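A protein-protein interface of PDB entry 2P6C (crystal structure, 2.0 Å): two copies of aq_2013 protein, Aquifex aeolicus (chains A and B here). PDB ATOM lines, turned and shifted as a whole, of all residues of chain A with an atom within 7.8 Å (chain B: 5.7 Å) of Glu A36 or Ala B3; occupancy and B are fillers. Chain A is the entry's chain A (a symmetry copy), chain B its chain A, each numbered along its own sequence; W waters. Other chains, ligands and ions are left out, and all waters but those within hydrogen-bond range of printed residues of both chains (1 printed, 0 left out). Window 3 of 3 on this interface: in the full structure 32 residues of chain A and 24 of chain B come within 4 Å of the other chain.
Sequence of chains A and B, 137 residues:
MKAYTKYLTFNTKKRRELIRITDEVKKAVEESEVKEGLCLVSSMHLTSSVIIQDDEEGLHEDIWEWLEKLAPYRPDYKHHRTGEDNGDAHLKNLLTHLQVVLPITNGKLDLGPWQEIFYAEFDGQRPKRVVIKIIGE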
ATOM      1  N   LYS A   2      17.343 -12.543  16.359  1.00  0.00           N
ATOM      2  CA  LYS A   2      17.439 -14.013  16.401  1.00  0.00           C
ATOM      3  C   LYS A   2      16.633 -14.676  15.261  1.00  0.00           C
ATOM      4  O   LYS A   2      15.579 -14.216  14.846  1.00  0.00           O
ATOM      5  CB  LYS A   2      16.851 -14.494  17.730  1.00  0.00           C
ATOM      6  CG  LYS A   2      17.731 -14.241  18.958  1.00  0.00           C
ATOM      7  CD  LYS A   2      17.042 -14.768  20.222  1.00  0.00           C
ATOM      8  CE  LYS A   2      17.894 -14.671  21.489  1.00  0.00           C
ATOM      9  NZ  LYS A   2      17.789 -13.327  22.035  1.00  0.00           N
ATOM     10  N   SER A  32      14.482 -21.898  19.873  1.00  0.00           N
ATOM     11  CA  SER A  32      14.866 -20.663  19.183  1.00  0.00           C
ATOM     12  C   SER A  32      15.194 -19.591  20.211  1.00  0.00           C
ATOM     13  O   SER A  32      15.862 -18.604  19.905  1.00  0.00           O
ATOM     14  CB  SER A  32      13.727 -20.150  18.300  1.00  0.00           C
ATOM     15  OG  SER A  32      12.810 -19.385  19.061  1.00  0.00           O
ATOM     16  N   GLU A  33      14.699 -19.795  21.428  1.00  0.00           N
ATOM     17  CA  GLU A  33      14.889 -18.867  22.538  1.00  0.00           C
ATOM     18  C   GLU A  33      14.259 -17.498  22.254  1.00  0.00           C
ATOM     19  O   GLU A  33      14.470 -16.526  22.967  1.00  0.00           O
ATOM     20  CB  GLU A  33      16.392 -18.721  22.783  1.00  0.00           C
ATOM     21  CG  GLU A  33      17.008 -19.991  23.373  1.00  0.00           C
ATOM     22  CD  GLU A  33      18.418 -19.703  23.831  1.00  0.00           C
ATOM     23  OE1 GLU A  33      19.184 -19.148  23.055  1.00  0.00           O
ATOM     24  OE2 GLU A  33      18.750 -20.058  24.960  1.00  0.00           O
ATOM     25  N   VAL A  34      13.463 -17.402  21.193  1.00  0.00           N
ATOM     26  CA  VAL A  34      12.782 -16.158  20.809  1.00  0.00           C
ATOM     27  C   VAL A  34      11.694 -15.856  21.854  1.00  0.00           C
ATOM     28  O   VAL A  34      10.955 -16.730  22.291  1.00  0.00           O
ATOM     29  CB  VAL A  34      12.237 -16.201  19.317  1.00  0.00           C
ATOM     30  CG1 VAL A  34      11.252 -15.055  19.089  1.00  0.00           C
ATOM     31  CG2 VAL A  34      13.391 -16.068  18.341  1.00  0.00           C
ATOM     32  N   LYS A  35      11.692 -14.656  22.317  1.00  0.00           N
ATOM     33  CA  LYS A  35      10.659 -14.096  23.247  1.00  0.00           C
ATOM     34  C   LYS A  35       9.526 -13.546  22.459  1.00  0.00           C
ATOM     35  O   LYS A  35       8.361 -13.770  22.756  1.00  0.00           O
ATOM     36  CB  LYS A  35      11.127 -12.916  24.144  1.00  0.00           C
ATOM     37  CG  LYS A  35      11.806 -13.400  25.428  1.00  0.00           C
ATOM     38  CD  LYS A  35      13.313 -13.133  25.421  1.00  0.00           C
ATOM     39  CE  LYS A  35      13.647 -11.642  25.308  1.00  0.00           C
ATOM     40  NZ  LYS A  35      15.057 -11.427  25.630  1.00  0.00           N
ATOM     41  N   GLU A  36       9.680 -12.741  21.541  1.00  0.00           N
ATOM     42  CA  GLU A  36       8.673 -12.050  20.753  1.00  0.00           C
ATOM     43  C   GLU A  36       9.062 -12.194  19.283  1.00  0.00           C
ATOM     44  O   GLU A  36      10.191 -11.884  18.909  1.00  0.00           O
ATOM     45  CB  GLU A  36       8.640 -10.568  21.137  1.00  0.00           C
ATOM     46  CG  GLU A  36       8.386 -10.288  22.617  1.00  0.00           C
ATOM     47  CD  GLU A  36       7.005 -10.712  23.076  1.00  0.00           C
ATOM     48  OE1 GLU A  36       6.049 -10.608  22.276  1.00  0.00           O
ATOM     49  OE2 GLU A  36       6.865 -11.130  24.246  1.00  0.00           O
ATOM     50  N   GLY A  37       8.145 -12.673  18.450  1.00  0.00           N
ATOM     51  CA  GLY A  37       8.484 -12.814  17.043  1.00  0.00           C
ATOM     52  C   GLY A  37       7.424 -13.446  16.166  1.00  0.00           C
ATOM     53  O   GLY A  37       6.243 -13.501  16.518  1.00  0.00           O
ATOM     54  N   LEU A  38       7.850 -13.901  14.996  1.00  0.00           N
ATOM     55  CA  LEU A  38       6.964 -14.542  14.054  1.00  0.00           C
ATOM     56  C   LEU A  38       7.471 -15.938  13.760  1.00  0.00           C
ATOM     57  O   LEU A  38       8.667 -16.200  13.737  1.00  0.00           O
ATOM     58  CB  LEU A  38       6.949 -13.714  12.767  1.00  0.00           C
ATOM     59  CG  LEU A  38       6.113 -12.441  12.900  1.00  0.00           C
ATOM     60  CD1 LEU A  38       6.058 -11.637  11.600  1.00  0.00           C
ATOM     61  CD2 LEU A  38       4.663 -12.721  13.296  1.00  0.00           C
ATOM     62  N   PRO A 103       2.281 -15.969  15.733  1.00  0.00           N
ATOM     63  CA  PRO A 103       2.944 -15.075  16.667  1.00  0.00           C
ATOM     64  C   PRO A 103       3.676 -15.850  17.753  1.00  0.00           C
ATOM     65  O   PRO A 103       3.314 -16.957  18.123  1.00  0.00           O
ATOM     66  CB  PRO A 103       1.881 -14.223  17.352  1.00  0.00           C
ATOM     67  CG  PRO A 103       0.497 -14.739  16.929  1.00  0.00           C
ATOM     68  CD  PRO A 103       0.857 -15.984  15.984  1.00  0.00           C
ATOM     69  N   ILE A 104       4.769 -15.248  18.235  1.00  0.00           N
ATOM     70  CA  ILE A 104       5.402 -15.760  19.425  1.00  0.00           C
ATOM     71  C   ILE A 104       5.324 -14.677  20.472  1.00  0.00           C
ATOM     72  O   ILE A 104       5.840 -13.581  20.298  1.00  0.00           O
ATOM     73  CB  ILE A 104       6.870 -16.056  19.107  1.00  0.00           C
ATOM     74  CG1 ILE A 104       6.986 -17.288  18.207  1.00  0.00           C
ATOM     75  CG2 ILE A 104       7.650 -16.351  20.408  1.00  0.00           C
ATOM     76  CD1 ILE A 104       8.398 -17.464  17.642  1.00  0.00           C
ATOM     77  N   THR A 105       4.647 -14.950  21.580  1.00  0.00           N
ATOM     78  CA  THR A 105       4.409 -13.961  22.607  1.00  0.00           C
ATOM     79  C   THR A 105       4.883 -14.485  23.963  1.00  0.00           C
ATOM     80  O   THR A 105       4.434 -15.512  24.453  1.00  0.00           O
ATOM     81  CB  THR A 105       2.904 -13.654  22.624  1.00  0.00           C
ATOM     82  OG1 THR A 105       2.484 -13.318  21.299  1.00  0.00           O
ATOM     83  CG2 THR A 105       2.625 -12.464  23.548  1.00  0.00           C
ATOM     84  N   ASN A 106       5.793 -13.775  24.618  1.00  0.00           N
ATOM     85  CA  ASN A 106       6.332 -14.156  25.916  1.00  0.00           C
ATOM     86  C   ASN A 106       6.932 -15.591  25.839  1.00  0.00           C
ATOM     87  O   ASN A 106       6.754 -16.415  26.727  1.00  0.00           O
ATOM     88  CB  ASN A 106       5.198 -14.046  26.983  1.00  0.00           C
ATOM     89  CG  ASN A 106       4.811 -12.588  27.316  1.00  0.00           C
ATOM     90  OD1 ASN A 106       5.616 -11.667  27.230  1.00  0.00           O
ATOM     91  ND2 ASN A 106       3.534 -12.415  27.696  1.00  0.00           N
ATOM     92  N   GLY A 107       7.666 -15.844  24.759  1.00  0.00           N
ATOM     93  CA  GLY A 107       8.347 -17.124  24.577  1.00  0.00           C
ATOM     94  C   GLY A 107       7.388 -18.301  24.309  1.00  0.00           C
ATOM     95  O   GLY A 107       7.691 -19.453  24.565  1.00  0.00           O
ATOM     96  N   LYS A 108       6.205 -17.935  23.776  1.00  0.00           N
ATOM     97  CA  LYS A 108       5.209 -18.963  23.516  1.00  0.00           C
ATOM     98  C   LYS A 108       4.491 -18.774  22.184  1.00  0.00           C
ATOM     99  O   LYS A 108       4.235 -17.664  21.736  1.00  0.00           O
ATOM    100  CB  LYS A 108       4.182 -18.882  24.627  1.00  0.00           C
ATOM    101  CG  LYS A 108       4.689 -19.552  25.895  1.00  0.00           C
ATOM    102  CD  LYS A 108       3.844 -19.185  27.109  1.00  0.00           C
ATOM    103  CE  LYS A 108       3.514 -17.690  27.167  1.00  0.00           C
ATOM    104  NZ  LYS A 108       2.445 -17.467  28.139  1.00  0.00           N
ATOM    105  N   ASP A 110       1.644 -18.232  20.130  1.00  0.00           N
ATOM    106  CA  ASP A 110       0.406 -17.491  20.446  1.00  0.00           C
ATOM    107  C   ASP A 110      -0.822 -18.095  19.742  1.00  0.00           C
ATOM    108  O   ASP A 110      -1.218 -17.652  18.668  1.00  0.00           O
ATOM    109  CB  ASP A 110       0.569 -16.029  20.009  1.00  0.00           C
ATOM    110  CG  ASP A 110      -0.256 -15.111  20.914  1.00  0.00           C
ATOM    111  OD1 ASP A 110      -1.178 -15.603  21.573  1.00  0.00           O
ATOM    112  OD2 ASP A 110       0.033 -13.919  20.946  1.00  0.00           O
ATOM    113  N   ILE A 134      11.711 -19.135  12.205  1.00  0.00           N
ATOM    114  CA  ILE A 134      11.413 -18.188  13.282  1.00  0.00           C
ATOM    115  C   ILE A 134      12.381 -17.017  13.284  1.00  0.00           C
ATOM    116  O   ILE A 134      13.581 -17.171  13.101  1.00  0.00           O
ATOM    117  CB  ILE A 134      11.548 -18.936  14.618  1.00  0.00           C
ATOM    118  CG1 ILE A 134      10.444 -20.008  14.689  1.00  0.00           C
ATOM    119  CG2 ILE A 134      11.331 -17.923  15.766  1.00  0.00           C
ATOM    120  CD1 ILE A 134      10.490 -21.001  15.865  1.00  0.00           C
ATOM    121  N   ILE A 135      11.842 -15.801  13.473  1.00  0.00           N
ATOM    122  CA  ILE A 135      12.662 -14.547  13.586  1.00  0.00           C
ATOM    123  C   ILE A 135      12.042 -13.729  14.704  1.00  0.00           C
ATOM    124  O   ILE A 135      10.840 -13.756  14.934  1.00  0.00           O
ATOM    125  CB  ILE A 135      12.841 -13.722  12.285  1.00  0.00           C
ATOM    126  CG1 ILE A 135      11.472 -13.187  11.754  1.00  0.00           C
ATOM    127  CG2 ILE A 135      13.491 -14.542  11.133  1.00  0.00           C
ATOM    128  CD1 ILE A 135      11.511 -12.093  10.642  1.00  0.00           C
ATOM    129  N   GLY A 136      12.864 -12.934  15.373  1.00  0.00           N
ATOM    130  CA  GLY A 136      12.376 -12.052  16.413  1.00  0.00           C
ATOM    131  C   GLY A 136      13.473 -11.934  17.446  1.00  0.00           C
ATOM    132  O   GLY A 136      14.658 -12.145  17.146  1.00  0.00           O
ATOM    133  N   GLU A 137      13.099 -11.606  18.679  1.00  0.00           N
ATOM    134  CA  GLU A 137      13.947 -11.367  19.844  1.00  0.00           C
ATOM    135  C   GLU A 137      13.454 -12.143  21.067  1.00  0.00           C
ATOM    136  O   GLU A 137      12.293 -12.080  21.452  1.00  0.00           O
ATOM    137  CB  GLU A 137      13.948  -9.862  20.136  1.00  0.00           C
ATOM    138  CG  GLU A 137      15.295  -9.367  20.679  1.00  0.00           C
ATOM    139  CD  GLU A 137      15.856  -8.303  19.756  1.00  0.00           C
ATOM    140  OE1 GLU A 137      15.452  -7.149  19.881  1.00  0.00           O
ATOM    141  OE2 GLU A 137      16.688  -8.631  18.922  1.00  0.00           O
ATOM    142  OXT GLU A 137      14.198 -12.864  21.721  1.00  0.00           O
ATOM    143  N   MET B   1      15.783  -5.508  18.086  1.00  0.00           N
ATOM    144  CA  MET B   1      14.612  -5.492  17.199  1.00  0.00           C
ATOM    145  C   MET B   1      13.328  -5.143  17.971  1.00  0.00           C
ATOM    146  O   MET B   1      13.177  -5.463  19.135  1.00  0.00           O
ATOM    147  CB  MET B   1      14.473  -6.898  16.608  1.00  0.00           C
ATOM    148  CG  MET B   1      13.056  -7.168  16.100  1.00  0.00           C
ATOM    149  SD  MET B   1      12.658  -8.915  15.987  1.00  0.00           S
ATOM    150  CE  MET B   1      12.853  -9.104  14.207  1.00  0.00           C
ATOM    151  N   LYS B   2      12.385  -4.426  17.288  1.00  0.00           N
ATOM    152  CA  LYS B   2      11.113  -4.032  17.921  1.00  0.00           C
ATOM    153  C   LYS B   2       9.986  -5.046  17.629  1.00  0.00           C
ATOM    154  O   LYS B   2       9.896  -5.644  16.565  1.00  0.00           O
ATOM    155  CB  LYS B   2      10.688  -2.680  17.341  1.00  0.00           C
ATOM    156  CG  LYS B   2      11.496  -1.477  17.841  1.00  0.00           C
ATOM    157  CD  LYS B   2      10.976  -0.186  17.198  1.00  0.00           C
ATOM    158  CE  LYS B   2      11.639   1.089  17.724  1.00  0.00           C
ATOM    159  NZ  LYS B   2      12.902   1.292  17.031  1.00  0.00           N
ATOM    160  N   ALA B   3       9.115  -5.266  18.609  1.00  0.00           N
ATOM    161  CA  ALA B   3       7.994  -6.195  18.512  1.00  0.00           C
ATOM    162  C   ALA B   3       6.839  -5.545  19.267  1.00  0.00           C
ATOM    163  O   ALA B   3       7.035  -4.903  20.302  1.00  0.00           O
ATOM    164  CB  ALA B   3       8.361  -7.528  19.130  1.00  0.00           C
ATOM    165  N   TYR B   4       5.637  -5.727  18.745  1.00  0.00           N
ATOM    166  CA  TYR B   4       4.468  -5.110  19.331  1.00  0.00           C
ATOM    167  C   TYR B   4       3.289  -6.060  19.168  1.00  0.00           C
ATOM    168  O   TYR B   4       3.077  -6.603  18.084  1.00  0.00           O
ATOM    169  CB  TYR B   4       4.224  -3.794  18.594  1.00  0.00           C
ATOM    170  CG  TYR B   4       3.050  -3.050  19.116  1.00  0.00           C
ATOM    171  CD1 TYR B   4       3.165  -2.282  20.267  1.00  0.00           C
ATOM    172  CD2 TYR B   4       1.786  -3.207  18.544  1.00  0.00           C
ATOM    173  CE1 TYR B   4       2.053  -1.701  20.854  1.00  0.00           C
ATOM    174  CE2 TYR B   4       0.658  -2.625  19.132  1.00  0.00           C
ATOM    175  CZ  TYR B   4       0.805  -1.879  20.295  1.00  0.00           C
ATOM    176  OH  TYR B   4      -0.286  -1.365  20.961  1.00  0.00           O
ATOM    177  N   THR B   5       2.536  -6.274  20.242  1.00  0.00           N
ATOM    178  CA  THR B   5       1.396  -7.168  20.192  1.00  0.00           C
ATOM    179  C   THR B   5       0.143  -6.464  20.678  1.00  0.00           C
ATOM    180  O   THR B   5       0.194  -5.675  21.621  1.00  0.00           O
ATOM    181  CB  THR B   5       1.647  -8.389  21.074  1.00  0.00           C
ATOM    182  OG1 THR B   5       2.903  -8.977  20.724  1.00  0.00           O
ATOM    183  CG2 THR B   5       0.544  -9.421  20.888  1.00  0.00           C
ATOM    184  N   VAL B  34       7.348   1.078  14.763  1.00  0.00           N
ATOM    185  CA  VAL B  34       8.118   0.357  13.740  1.00  0.00           C
ATOM    186  C   VAL B  34       8.140   1.209  12.458  1.00  0.00           C
ATOM    187  O   VAL B  34       7.139   1.776  12.041  1.00  0.00           O
ATOM    188  CB  VAL B  34       7.586  -1.123  13.512  1.00  0.00           C
ATOM    189  CG1 VAL B  34       8.173  -1.694  12.223  1.00  0.00           C
ATOM    190  CG2 VAL B  34       7.993  -2.004  14.678  1.00  0.00           C
ATOM    191  N   LYS B 133       0.423  -8.889  15.326  1.00  0.00           N
ATOM    192  CA  LYS B 133       1.787  -9.045  15.775  1.00  0.00           C
ATOM    193  C   LYS B 133       2.727  -8.374  14.790  1.00  0.00           C
ATOM    194  O   LYS B 133       2.764  -8.696  13.609  1.00  0.00           O
ATOM    195  CB  LYS B 133       2.094 -10.540  15.851  1.00  0.00           C
ATOM    196  CG  LYS B 133       3.422 -10.820  16.558  1.00  0.00           C
ATOM    197  CD  LYS B 133       3.364 -10.482  18.047  1.00  0.00           C
ATOM    198  CE  LYS B 133       4.381 -11.289  18.866  1.00  0.00           C
ATOM    199  NZ  LYS B 133       3.979 -11.305  20.271  1.00  0.00           N
ATOM    200  N   ILE B 134       3.441  -7.365  15.336  1.00  0.00           N
ATOM    201  CA  ILE B 134       4.367  -6.569  14.527  1.00  0.00           C
ATOM    202  C   ILE B 134       5.808  -6.761  14.968  1.00  0.00           C
ATOM    203  O   ILE B 134       6.122  -6.804  16.150  1.00  0.00           O
ATOM    204  CB  ILE B 134       3.996  -5.089  14.705  1.00  0.00           C
ATOM    205  CG1 ILE B 134       2.602  -4.858  14.090  1.00  0.00           C
ATOM    206  CG2 ILE B 134       5.026  -4.232  13.933  1.00  0.00           C
ATOM    207  CD1 ILE B 134       1.946  -3.482  14.307  1.00  0.00           C
ATOM    208  N   ILE B 135       6.714  -6.909  13.988  1.00  0.00           N
ATOM    209  CA  ILE B 135       8.191  -7.027  14.245  1.00  0.00           C
ATOM    210  C   ILE B 135       8.879  -6.188  13.183  1.00  0.00           C
ATOM    211  O   ILE B 135       8.411  -6.056  12.060  1.00  0.00           O
ATOM    212  CB  ILE B 135       8.764  -8.466  14.316  1.00  0.00           C
ATOM    213  CG1 ILE B 135       8.595  -9.218  12.958  1.00  0.00           C
ATOM    214  CG2 ILE B 135       8.081  -9.335  15.412  1.00  0.00           C
ATOM    215  CD1 ILE B 135       9.387 -10.549  12.769  1.00  0.00           C
ATOM    216  N   GLY B 136      10.046  -5.658  13.521  1.00  0.00           N
ATOM    217  CA  GLY B 136      10.830  -4.899  12.568  1.00  0.00           C
ATOM    218  C   GLY B 136      11.567  -3.835  13.350  1.00  0.00           C
ATOM    219  O   GLY B 136      11.802  -3.979  14.559  1.00  0.00           O
HETATM  220  O   HOH W   1       5.010  -7.635  21.916  1.00  0.00           O
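The backbone carbonyl oxygen of Ile A135 lies within hydrogen-bond range of the backbone NH of Leu A38 (3.0 Å). The backbone NH (N) of Lys A2 lies within hydrogen-bond range of the backbone carbonyl oxygen (O) of Gly A136, at 2.8 Å. The backbone carbonyl oxygen (O) of Gly A37 is in hydrogen-bond range of the backbone NH (N) of Ile A104. OG1 of Thr B5 sits at hydrogen-bond distance from NZ of Lys B133, at 2.6 Å. O of Glu A137 lies within hydrogen-bond range of N of Lys A35 (2.8 Å). The chain-end carboxylate of Glu A137 sits at hydrogen-bond distance from the backbone NH of Glu A36 (2.7 Å).
Among the printed residues, merely in contact across the chains: Glu A36 with Ala B3, Glu A36 with Thr B5, Gly A37 with Lys B133, Gly A37 with Ile B135, Leu A38 with Lys B133, Leu A38 with Ile B135, Pro A103 with Lys B133, Ile A135 with Ile B135 and Gly A136 with Met B1.
Ile B135 touches its own counterpart, Ile A135. Of the 13 pairs that touch across the chains among the printed residues, 1 has its exchanged pair printed and touching as well.
Glu A36 touches just these residues of chain B: Ala B3 (3.7 Å), Thr B5 (3.9 Å) and Lys B133 (3.0 Å). Ala B3 touches just one residue of chain A: Glu A36. Of the printed residues of chain B, Pro A103 touches Lys B133 (3.8 Å). Of the printed residues of chain B, Leu A38 touches Lys B133 and Ile B135. Ile B134 touches none of the printed residues of chain A. Tyr B4 touches none of the printed residues of chain A. The nearest printed residue of chain B that does not touch Glu A36 is Ile B135 (4.8 Å).
Water W1 bridges OG1 of Thr B5 (2.8 Å) and OE1 of Glu A36 (3.2 Å).
The side-chain amino group (NZ) of Lys B133 lies within hydrogen-bond range of the side-chain hydroxyl (OG1) of Thr A105 (2.7 Å). The side-chain carboxylate (OE1) of Glu A137 is in hydrogen-bond range of the backbone NH (N) of Met B1 (2.5 Å). NZ of Lys B133 lies within salt-bridge range of OE1 of Glu A36, at 3.0 Å. NZ of Lys B133 is in hydrogen-bond range of O of Ile A104, at 2.9 Å.
Of the 19 printed residues of chain A, 9 touch a printed residue of chain B. Printed residues of chain A that touch a printed residue of chain B: Glu A36, Gly A37, Leu A38, Pro A103, Ile A104, Thr A105, Ile A135, Gly A136 and Glu A137. Hydrophobic or aromatic side chains of chain B within 4 Å of the printed part of chain A: Met B1, Ala B3 and Ile B135.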
